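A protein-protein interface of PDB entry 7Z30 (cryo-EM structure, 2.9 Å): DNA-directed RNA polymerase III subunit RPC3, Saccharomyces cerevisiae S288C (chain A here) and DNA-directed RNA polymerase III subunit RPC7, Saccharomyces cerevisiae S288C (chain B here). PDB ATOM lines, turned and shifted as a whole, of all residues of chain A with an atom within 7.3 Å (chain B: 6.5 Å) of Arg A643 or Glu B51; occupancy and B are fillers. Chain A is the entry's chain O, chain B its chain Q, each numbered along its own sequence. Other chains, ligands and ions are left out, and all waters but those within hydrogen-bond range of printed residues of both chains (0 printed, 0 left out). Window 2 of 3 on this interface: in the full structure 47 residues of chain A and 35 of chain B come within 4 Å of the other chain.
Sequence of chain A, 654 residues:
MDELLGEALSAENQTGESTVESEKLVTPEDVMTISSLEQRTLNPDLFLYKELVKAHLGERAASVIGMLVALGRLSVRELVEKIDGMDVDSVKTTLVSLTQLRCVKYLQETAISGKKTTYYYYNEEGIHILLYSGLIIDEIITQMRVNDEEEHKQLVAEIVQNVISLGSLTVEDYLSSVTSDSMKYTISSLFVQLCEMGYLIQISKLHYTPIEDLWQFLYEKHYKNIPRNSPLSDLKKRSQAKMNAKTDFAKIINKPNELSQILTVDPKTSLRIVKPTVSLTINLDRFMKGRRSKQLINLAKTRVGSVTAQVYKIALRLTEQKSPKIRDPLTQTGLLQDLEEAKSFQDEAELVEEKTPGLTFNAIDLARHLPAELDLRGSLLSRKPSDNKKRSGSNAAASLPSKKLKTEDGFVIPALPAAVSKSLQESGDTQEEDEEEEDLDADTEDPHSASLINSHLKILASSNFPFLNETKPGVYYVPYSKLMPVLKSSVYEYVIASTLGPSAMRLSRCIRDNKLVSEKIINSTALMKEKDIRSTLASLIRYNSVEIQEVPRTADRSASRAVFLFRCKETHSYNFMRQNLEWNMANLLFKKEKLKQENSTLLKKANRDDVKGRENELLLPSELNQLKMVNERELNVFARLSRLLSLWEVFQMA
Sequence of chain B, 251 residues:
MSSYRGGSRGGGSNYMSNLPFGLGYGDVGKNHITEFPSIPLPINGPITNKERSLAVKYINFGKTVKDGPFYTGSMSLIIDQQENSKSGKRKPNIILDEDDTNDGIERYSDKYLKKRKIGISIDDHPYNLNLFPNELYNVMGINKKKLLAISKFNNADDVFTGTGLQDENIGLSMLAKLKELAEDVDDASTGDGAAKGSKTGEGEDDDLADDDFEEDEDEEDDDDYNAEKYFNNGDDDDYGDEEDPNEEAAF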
ATOM      1  N   LEU A 135     -20.207   4.044  -9.056  1.00  0.00           N
ATOM      2  CA  LEU A 135     -20.212   2.658  -9.510  1.00  0.00           C
ATOM      3  C   LEU A 135     -20.245   2.580 -11.029  1.00  0.00           C
ATOM      4  O   LEU A 135     -19.647   1.673 -11.622  1.00  0.00           O
ATOM      5  CB  LEU A 135     -21.391   1.896  -8.907  1.00  0.00           C
ATOM      6  CG  LEU A 135     -21.684   2.074  -7.418  1.00  0.00           C
ATOM      7  CD1 LEU A 135     -22.788   1.117  -7.001  1.00  0.00           C
ATOM      8  CD2 LEU A 135     -20.433   1.839  -6.585  1.00  0.00           C
ATOM      9  N   LEU A 635     -15.150  10.946   3.682  1.00  0.00           N
ATOM     10  CA  LEU A 635     -14.691   9.699   3.075  1.00  0.00           C
ATOM     11  C   LEU A 635     -15.370   8.492   3.712  1.00  0.00           C
ATOM     12  O   LEU A 635     -15.762   7.550   3.014  1.00  0.00           O
ATOM     13  CB  LEU A 635     -13.173   9.585   3.195  1.00  0.00           C
ATOM     14  CG  LEU A 635     -12.380   9.794   1.905  1.00  0.00           C
ATOM     15  CD1 LEU A 635     -12.357  11.262   1.523  1.00  0.00           C
ATOM     16  CD2 LEU A 635     -10.966   9.257   2.060  1.00  0.00           C
ATOM     17  N   VAL A 637     -18.332   8.482   5.203  1.00  0.00           N
ATOM     18  CA  VAL A 637     -19.737   8.456   4.807  1.00  0.00           C
ATOM     19  C   VAL A 637     -19.880   7.965   3.371  1.00  0.00           C
ATOM     20  O   VAL A 637     -20.835   7.257   3.039  1.00  0.00           O
ATOM     21  CB  VAL A 637     -20.409   9.829   5.023  1.00  0.00           C
ATOM     22  CG1 VAL A 637     -20.212  10.754   3.834  1.00  0.00           C
ATOM     23  CG2 VAL A 637     -21.894   9.640   5.282  1.00  0.00           C
ATOM     24  N   PHE A 638     -18.922   8.302   2.500  1.00  0.00           N
ATOM     25  CA  PHE A 638     -18.965   7.791   1.133  1.00  0.00           C
ATOM     26  C   PHE A 638     -18.709   6.290   1.095  1.00  0.00           C
ATOM     27  O   PHE A 638     -19.322   5.572   0.298  1.00  0.00           O
ATOM     28  CB  PHE A 638     -17.958   8.530   0.255  1.00  0.00           C
ATOM     29  CG  PHE A 638     -18.511   9.766  -0.393  1.00  0.00           C
ATOM     30  CD1 PHE A 638     -19.651   9.698  -1.177  1.00  0.00           C
ATOM     31  CD2 PHE A 638     -17.888  10.990  -0.230  1.00  0.00           C
ATOM     32  CE1 PHE A 638     -20.164  10.832  -1.779  1.00  0.00           C
ATOM     33  CE2 PHE A 638     -18.395  12.126  -0.831  1.00  0.00           C
ATOM     34  CZ  PHE A 638     -19.531  12.046  -1.608  1.00  0.00           C
ATOM     35  N   ALA A 639     -17.798   5.802   1.937  1.00  0.00           N
ATOM     36  CA  ALA A 639     -17.567   4.362   2.019  1.00  0.00           C
ATOM     37  C   ALA A 639     -18.815   3.633   2.497  1.00  0.00           C
ATOM     38  O   ALA A 639     -19.174   2.582   1.954  1.00  0.00           O
ATOM     39  CB  ALA A 639     -16.385   4.071   2.942  1.00  0.00           C
ATOM     40  N   ARG A 640     -19.491   4.180   3.511  1.00  0.00           N
ATOM     41  CA  ARG A 640     -20.745   3.592   3.971  1.00  0.00           C
ATOM     42  C   ARG A 640     -21.807   3.637   2.880  1.00  0.00           C
ATOM     43  O   ARG A 640     -22.567   2.679   2.703  1.00  0.00           O
ATOM     44  CB  ARG A 640     -21.238   4.311   5.228  1.00  0.00           C
ATOM     45  CG  ARG A 640     -21.060   3.515   6.509  1.00  0.00           C
ATOM     46  CD  ARG A 640     -19.798   3.922   7.239  1.00  0.00           C
ATOM     47  NE  ARG A 640     -19.802   5.343   7.566  1.00  0.00           N
ATOM     48  CZ  ARG A 640     -18.898   5.938   8.333  1.00  0.00           C
ATOM     49  NH1 ARG A 640     -17.892   5.263   8.866  1.00  0.00           N
ATOM     50  NH2 ARG A 640     -19.009   7.240   8.572  1.00  0.00           N
ATOM     51  N   LEU A 641     -21.871   4.745   2.139  1.00  0.00           N
ATOM     52  CA  LEU A 641     -22.815   4.863   1.033  1.00  0.00           C
ATOM     53  C   LEU A 641     -22.565   3.785  -0.013  1.00  0.00           C
ATOM     54  O   LEU A 641     -23.498   3.122  -0.476  1.00  0.00           O
ATOM     55  CB  LEU A 641     -22.694   6.257   0.411  1.00  0.00           C
ATOM     56  CG  LEU A 641     -23.841   6.895  -0.378  1.00  0.00           C
ATOM     57  CD1 LEU A 641     -23.475   8.334  -0.687  1.00  0.00           C
ATOM     58  CD2 LEU A 641     -24.165   6.146  -1.662  1.00  0.00           C
ATOM     59  N   SER A 642     -21.300   3.591  -0.390  1.00  0.00           N
ATOM     60  CA  SER A 642     -20.973   2.595  -1.404  1.00  0.00           C
ATOM     61  C   SER A 642     -21.246   1.184  -0.901  1.00  0.00           C
ATOM     62  O   SER A 642     -21.721   0.327  -1.658  1.00  0.00           O
ATOM     63  CB  SER A 642     -19.512   2.745  -1.829  1.00  0.00           C
ATOM     64  OG  SER A 642     -19.110   4.102  -1.786  1.00  0.00           O
ATOM     65  N   ARG A 643     -20.949   0.920   0.374  1.00  0.00           N
ATOM     66  CA  ARG A 643     -21.195  -0.407   0.929  1.00  0.00           C
ATOM     67  C   ARG A 643     -22.689  -0.693   1.026  1.00  0.00           C
ATOM     68  O   ARG A 643     -23.118  -1.844   0.879  1.00  0.00           O
ATOM     69  CB  ARG A 643     -20.522  -0.526   2.295  1.00  0.00           C
ATOM     70  CG  ARG A 643     -20.361  -1.949   2.787  1.00  0.00           C
ATOM     71  CD  ARG A 643     -19.043  -2.128   3.531  1.00  0.00           C
ATOM     72  NE  ARG A 643     -17.882  -1.921   2.674  1.00  0.00           N
ATOM     73  CZ  ARG A 643     -17.497  -2.748   1.711  1.00  0.00           C
ATOM     74  NH1 ARG A 643     -18.152  -3.868   1.459  1.00  0.00           N
ATOM     75  NH2 ARG A 643     -16.425  -2.446   0.986  1.00  0.00           N
ATOM     76  N   LEU A 644     -23.494   0.341   1.276  1.00  0.00           N
ATOM     77  CA  LEU A 644     -24.944   0.195   1.228  1.00  0.00           C
ATOM     78  C   LEU A 644     -25.448   0.068  -0.205  1.00  0.00           C
ATOM     79  O   LEU A 644     -26.502  -0.533  -0.443  1.00  0.00           O
ATOM     80  CB  LEU A 644     -25.603   1.384   1.928  1.00  0.00           C
ATOM     81  CG  LEU A 644     -26.951   1.182   2.621  1.00  0.00           C
ATOM     82  CD1 LEU A 644     -27.135   2.204   3.728  1.00  0.00           C
ATOM     83  CD2 LEU A 644     -28.073   1.299   1.611  1.00  0.00           C
ATOM     84  N   LEU A 645     -24.703   0.613  -1.170  1.00  0.00           N
ATOM     85  CA  LEU A 645     -25.125   0.621  -2.566  1.00  0.00           C
ATOM     86  C   LEU A 645     -25.106  -0.761  -3.207  1.00  0.00           C
ATOM     87  O   LEU A 645     -25.357  -0.866  -4.413  1.00  0.00           O
ATOM     88  CB  LEU A 645     -24.232   1.573  -3.365  1.00  0.00           C
ATOM     89  CG  LEU A 645     -24.927   2.570  -4.294  1.00  0.00           C
ATOM     90  CD1 LEU A 645     -26.073   3.240  -3.581  1.00  0.00           C
ATOM     91  CD2 LEU A 645     -23.939   3.615  -4.773  1.00  0.00           C
ATOM     92  N   SER A 646     -24.817  -1.811  -2.443  1.00  0.00           N
ATOM     93  CA  SER A 646     -24.900  -3.181  -2.927  1.00  0.00           C
ATOM     94  C   SER A 646     -26.140  -3.905  -2.409  1.00  0.00           C
ATOM     95  O   SER A 646     -26.216  -5.135  -2.509  1.00  0.00           O
ATOM     96  CB  SER A 646     -23.637  -3.953  -2.540  1.00  0.00           C
ATOM     97  OG  SER A 646     -23.521  -4.066  -1.132  1.00  0.00           O
ATOM     98  N   LEU A 647     -27.111  -3.168  -1.866  1.00  0.00           N
ATOM     99  CA  LEU A 647     -28.226  -3.770  -1.146  1.00  0.00           C
ATOM    100  C   LEU A 647     -29.606  -3.477  -1.717  1.00  0.00           C
ATOM    101  O   LEU A 647     -30.490  -4.326  -1.572  1.00  0.00           O
ATOM    102  CB  LEU A 647     -28.215  -3.325   0.326  1.00  0.00           C
ATOM    103  CG  LEU A 647     -27.469  -4.202   1.335  1.00  0.00           C
ATOM    104  CD1 LEU A 647     -27.998  -5.626   1.300  1.00  0.00           C
ATOM    105  CD2 LEU A 647     -25.969  -4.175   1.086  1.00  0.00           C
ATOM    106  N   PRO B  42     -23.393  -3.966   9.723  1.00  0.00           N
ATOM    107  CA  PRO B  42     -22.016  -4.308   9.338  1.00  0.00           C
ATOM    108  C   PRO B  42     -21.542  -3.701   8.026  1.00  0.00           C
ATOM    109  O   PRO B  42     -20.517  -4.147   7.501  1.00  0.00           O
ATOM    110  CB  PRO B  42     -22.083  -5.837   9.222  1.00  0.00           C
ATOM    111  CG  PRO B  42     -23.473  -6.103   8.767  1.00  0.00           C
ATOM    112  CD  PRO B  42     -24.342  -5.049   9.407  1.00  0.00           C
ATOM    113  N   ILE B  43     -22.245  -2.708   7.488  1.00  0.00           N
ATOM    114  CA  ILE B  43     -21.852  -2.059   6.246  1.00  0.00           C
ATOM    115  C   ILE B  43     -20.831  -0.946   6.496  1.00  0.00           C
ATOM    116  O   ILE B  43     -20.498  -0.193   5.582  1.00  0.00           O
ATOM    117  CB  ILE B  43     -23.075  -1.545   5.470  1.00  0.00           C
ATOM    118  CG1 ILE B  43     -23.680  -0.306   6.136  1.00  0.00           C
ATOM    119  CG2 ILE B  43     -24.123  -2.640   5.344  1.00  0.00           C
ATOM    120  CD1 ILE B  43     -23.413   0.990   5.399  1.00  0.00           C
ATOM    121  N   ASN B  44     -20.313  -0.846   7.718  1.00  0.00           N
ATOM    122  CA  ASN B  44     -19.310   0.147   8.088  1.00  0.00           C
ATOM    123  C   ASN B  44     -17.961  -0.513   8.363  1.00  0.00           C
ATOM    124  O   ASN B  44     -17.278  -0.189   9.337  1.00  0.00           O
ATOM    125  CB  ASN B  44     -19.770   0.951   9.301  1.00  0.00           C
ATOM    126  CG  ASN B  44     -20.401   0.082  10.365  1.00  0.00           C
ATOM    127  OD1 ASN B  44     -20.170  -1.126  10.409  1.00  0.00           O
ATOM    128  ND2 ASN B  44     -21.208   0.689  11.228  1.00  0.00           N
ATOM    129  N   GLY B  45     -17.567  -1.455   7.502  1.00  0.00           N
ATOM    130  CA  GLY B  45     -16.344  -2.180   7.688  1.00  0.00           C
ATOM    131  C   GLY B  45     -15.122  -1.346   7.345  1.00  0.00           C
ATOM    132  O   GLY B  45     -15.216  -0.151   7.032  1.00  0.00           O
ATOM    133  N   PRO B  46     -13.950  -1.979   7.411  1.00  0.00           N
ATOM    134  CA  PRO B  46     -12.701  -1.255   7.143  1.00  0.00           C
ATOM    135  C   PRO B  46     -12.639  -0.741   5.711  1.00  0.00           C
ATOM    136  O   PRO B  46     -13.205  -1.333   4.790  1.00  0.00           O
ATOM    137  CB  PRO B  46     -11.617  -2.307   7.408  1.00  0.00           C
ATOM    138  CG  PRO B  46     -12.273  -3.318   8.298  1.00  0.00           C
ATOM    139  CD  PRO B  46     -13.705  -3.360   7.859  1.00  0.00           C
ATOM    140  N   ILE B  47     -11.940   0.382   5.535  1.00  0.00           N
ATOM    141  CA  ILE B  47     -11.794   0.974   4.211  1.00  0.00           C
ATOM    142  C   ILE B  47     -10.533   0.442   3.531  1.00  0.00           C
ATOM    143  O   ILE B  47      -9.514   0.153   4.169  1.00  0.00           O
ATOM    144  CB  ILE B  47     -11.776   2.510   4.308  1.00  0.00           C
ATOM    145  CG1 ILE B  47     -12.006   3.144   2.936  1.00  0.00           C
ATOM    146  CG2 ILE B  47     -10.474   3.006   4.928  1.00  0.00           C
ATOM    147  CD1 ILE B  47     -12.098   4.654   2.966  1.00  0.00           C
ATOM    148  N   THR B  48     -10.618   0.284   2.213  1.00  0.00           N
ATOM    149  CA  THR B  48      -9.472  -0.091   1.398  1.00  0.00           C
ATOM    150  C   THR B  48      -9.183   1.003   0.377  1.00  0.00           C
ATOM    151  O   THR B  48      -9.862   2.034   0.316  1.00  0.00           O
ATOM    152  CB  THR B  48      -9.692  -1.435   0.685  1.00  0.00           C
ATOM    153  OG1 THR B  48     -10.704  -1.297  -0.321  1.00  0.00           O
ATOM    154  CG2 THR B  48     -10.113  -2.509   1.678  1.00  0.00           C
ATOM    155  N   ASN B  49      -8.145   0.760  -0.427  1.00  0.00           N
ATOM    156  CA  ASN B  49      -7.745   1.728  -1.442  1.00  0.00           C
ATOM    157  C   ASN B  49      -8.849   1.936  -2.471  1.00  0.00           C
ATOM    158  O   ASN B  49      -9.101   3.067  -2.904  1.00  0.00           O
ATOM    159  CB  ASN B  49      -6.451   1.271  -2.117  1.00  0.00           C
ATOM    160  CG  ASN B  49      -6.014   2.198  -3.232  1.00  0.00           C
ATOM    161  OD1 ASN B  49      -6.084   3.420  -3.101  1.00  0.00           O
ATOM    162  ND2 ASN B  49      -5.550   1.621  -4.335  1.00  0.00           N
ATOM    163  N   LYS B  50      -9.521   0.855  -2.874  1.00  0.00           N
ATOM    164  CA  LYS B  50     -10.628   0.984  -3.816  1.00  0.00           C
ATOM    165  C   LYS B  50     -11.760   1.819  -3.232  1.00  0.00           C
ATOM    166  O   LYS B  50     -12.365   2.632  -3.938  1.00  0.00           O
ATOM    167  CB  LYS B  50     -11.138  -0.399  -4.227  1.00  0.00           C
ATOM    168  CG  LYS B  50     -10.580  -0.902  -5.551  1.00  0.00           C
ATOM    169  CD  LYS B  50     -11.365  -2.104  -6.061  1.00  0.00           C
ATOM    170  CE  LYS B  50     -10.772  -2.645  -7.352  1.00  0.00           C
ATOM    171  NZ  LYS B  50     -10.635  -1.583  -8.390  1.00  0.00           N
ATOM    172  N   GLU B  51     -12.068   1.631  -1.947  1.00  0.00           N
ATOM    173  CA  GLU B  51     -13.130   2.419  -1.324  1.00  0.00           C
ATOM    174  C   GLU B  51     -12.747   3.889  -1.220  1.00  0.00           C
ATOM    175  O   GLU B  51     -13.580   4.776  -1.459  1.00  0.00           O
ATOM    176  CB  GLU B  51     -13.482   1.845   0.046  1.00  0.00           C
ATOM    177  CG  GLU B  51     -13.243   0.358   0.162  1.00  0.00           C
ATOM    178  CD  GLU B  51     -14.444  -0.457  -0.268  1.00  0.00           C
ATOM    179  OE1 GLU B  51     -14.448  -1.683  -0.030  1.00  0.00           O
ATOM    180  OE2 GLU B  51     -15.386   0.127  -0.845  1.00  0.00           O
ATOM    181  N   ARG B  52     -11.493   4.170  -0.866  1.00  0.00           N
ATOM    182  CA  ARG B  52     -11.037   5.555  -0.844  1.00  0.00           C
ATOM    183  C   ARG B  52     -11.115   6.174  -2.236  1.00  0.00           C
ATOM    184  O   ARG B  52     -11.476   7.348  -2.387  1.00  0.00           O
ATOM    185  CB  ARG B  52      -9.615   5.623  -0.290  1.00  0.00           C
ATOM    186  CG  ARG B  52      -9.050   7.023  -0.166  1.00  0.00           C
ATOM    187  CD  ARG B  52      -7.694   6.990   0.517  1.00  0.00           C
ATOM    188  NE  ARG B  52      -7.771   7.464   1.894  1.00  0.00           N
ATOM    189  CZ  ARG B  52      -8.031   6.691   2.939  1.00  0.00           C
ATOM    190  NH1 ARG B  52      -8.242   5.391   2.803  1.00  0.00           N
ATOM    191  NH2 ARG B  52      -8.081   7.234   4.152  1.00  0.00           N
ATOM    192  N   SER B  53     -10.796   5.390  -3.269  1.00  0.00           N
ATOM    193  CA  SER B  53     -10.918   5.877  -4.639  1.00  0.00           C
ATOM    194  C   SER B  53     -12.373   6.134  -5.020  1.00  0.00           C
ATOM    195  O   SER B  53     -12.659   7.103  -5.733  1.00  0.00           O
ATOM    196  CB  SER B  53     -10.272   4.884  -5.604  1.00  0.00           C
ATOM    197  OG  SER B  53     -10.728   5.080  -6.930  1.00  0.00           O
ATOM    198  N   LEU B  54     -13.299   5.273  -4.578  1.00  0.00           N
ATOM    199  CA  LEU B  54     -14.719   5.544  -4.798  1.00  0.00           C
ATOM    200  C   LEU B  54     -15.134   6.852  -4.141  1.00  0.00           C
ATOM    201  O   LEU B  54     -15.876   7.644  -4.730  1.00  0.00           O
ATOM    202  CB  LEU B  54     -15.596   4.398  -4.281  1.00  0.00           C
ATOM    203  CG  LEU B  54     -15.531   2.980  -4.848  1.00  0.00           C
ATOM    204  CD1 LEU B  54     -15.452   1.948  -3.755  1.00  0.00           C
ATOM    205  CD2 LEU B  54     -16.781   2.723  -5.660  1.00  0.00           C
ATOM    206  N   ALA B  55     -14.659   7.099  -2.919  1.00  0.00           N
ATOM    207  CA  ALA B  55     -14.973   8.362  -2.257  1.00  0.00           C
ATOM    208  C   ALA B  55     -14.412   9.550  -3.035  1.00  0.00           C
ATOM    209  O   ALA B  55     -15.084  10.580  -3.192  1.00  0.00           O
ATOM    210  CB  ALA B  55     -14.437   8.353  -0.827  1.00  0.00           C
ATOM    211  N   VAL B  56     -13.178   9.423  -3.531  1.00  0.00           N
ATOM    212  CA  VAL B  56     -12.544  10.525  -4.251  1.00  0.00           C
ATOM    213  C   VAL B  56     -13.297  10.825  -5.544  1.00  0.00           C
ATOM    214  O   VAL B  56     -13.594  11.983  -5.859  1.00  0.00           O
ATOM    215  CB  VAL B  56     -11.062  10.211  -4.519  1.00  0.00           C
ATOM    216  CG1 VAL B  56     -10.492  11.176  -5.547  1.00  0.00           C
ATOM    217  CG2 VAL B  56     -10.264  10.279  -3.226  1.00  0.00           C
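The side-chain carboxylate (OE2) of Glu B51 is in salt-bridge range of the guanidinium group (NH2) of Arg A643 (3.3 Å).
Among the printed residues, pairs that only touch across the chains: Leu A135 with Leu B54 (3.9 Å), Leu A635 with Arg B52 (3.7 Å), Leu A635 with Ala B55 (3.7 Å), Phe A638 with Ala B55 (3.7 Å), Arg A640 with Ile B43 (3.3 Å), Arg A640 with Asn B44 (3.6 Å) and Arg A643 with Ile B43 (3.2 Å).
The backbone carbonyl oxygen (O) of Arg A643 is in hydrogen-bond range of the side-chain hydroxyl (OG) of Ser A646, at 3.0 Å. The backbone carbonyl oxygen (O) of Phe A638 lies within hydrogen-bond range of the side-chain hydroxyl (OG) of Ser A642.
Of the printed residues of chain B, Leu A135 touches Leu B54. Printed residues of chain A within 4 Å of Ile B43: Arg A640 (3.3 Å) and Arg A643 (3.2 Å). Glu B51 touches just one residue of chain A: Arg A643. Of the printed residues of chain A, Arg B52 touches Leu A635. The nearest printed residue of chain B that does not touch Leu A635 is Ile B47 (4.7 Å).
Of the 15 printed residues of chain B, 6 touch a printed residue of chain A. Of the 13 printed residues of chain A, 5 touch a printed residue of chain B. Hydrophobic or aromatic side chains of chain A within 4 Å of the printed part of chain B: Leu A135, Leu A635 and Phe A638. Among the printed residues, 8 pairs touch across the chains.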
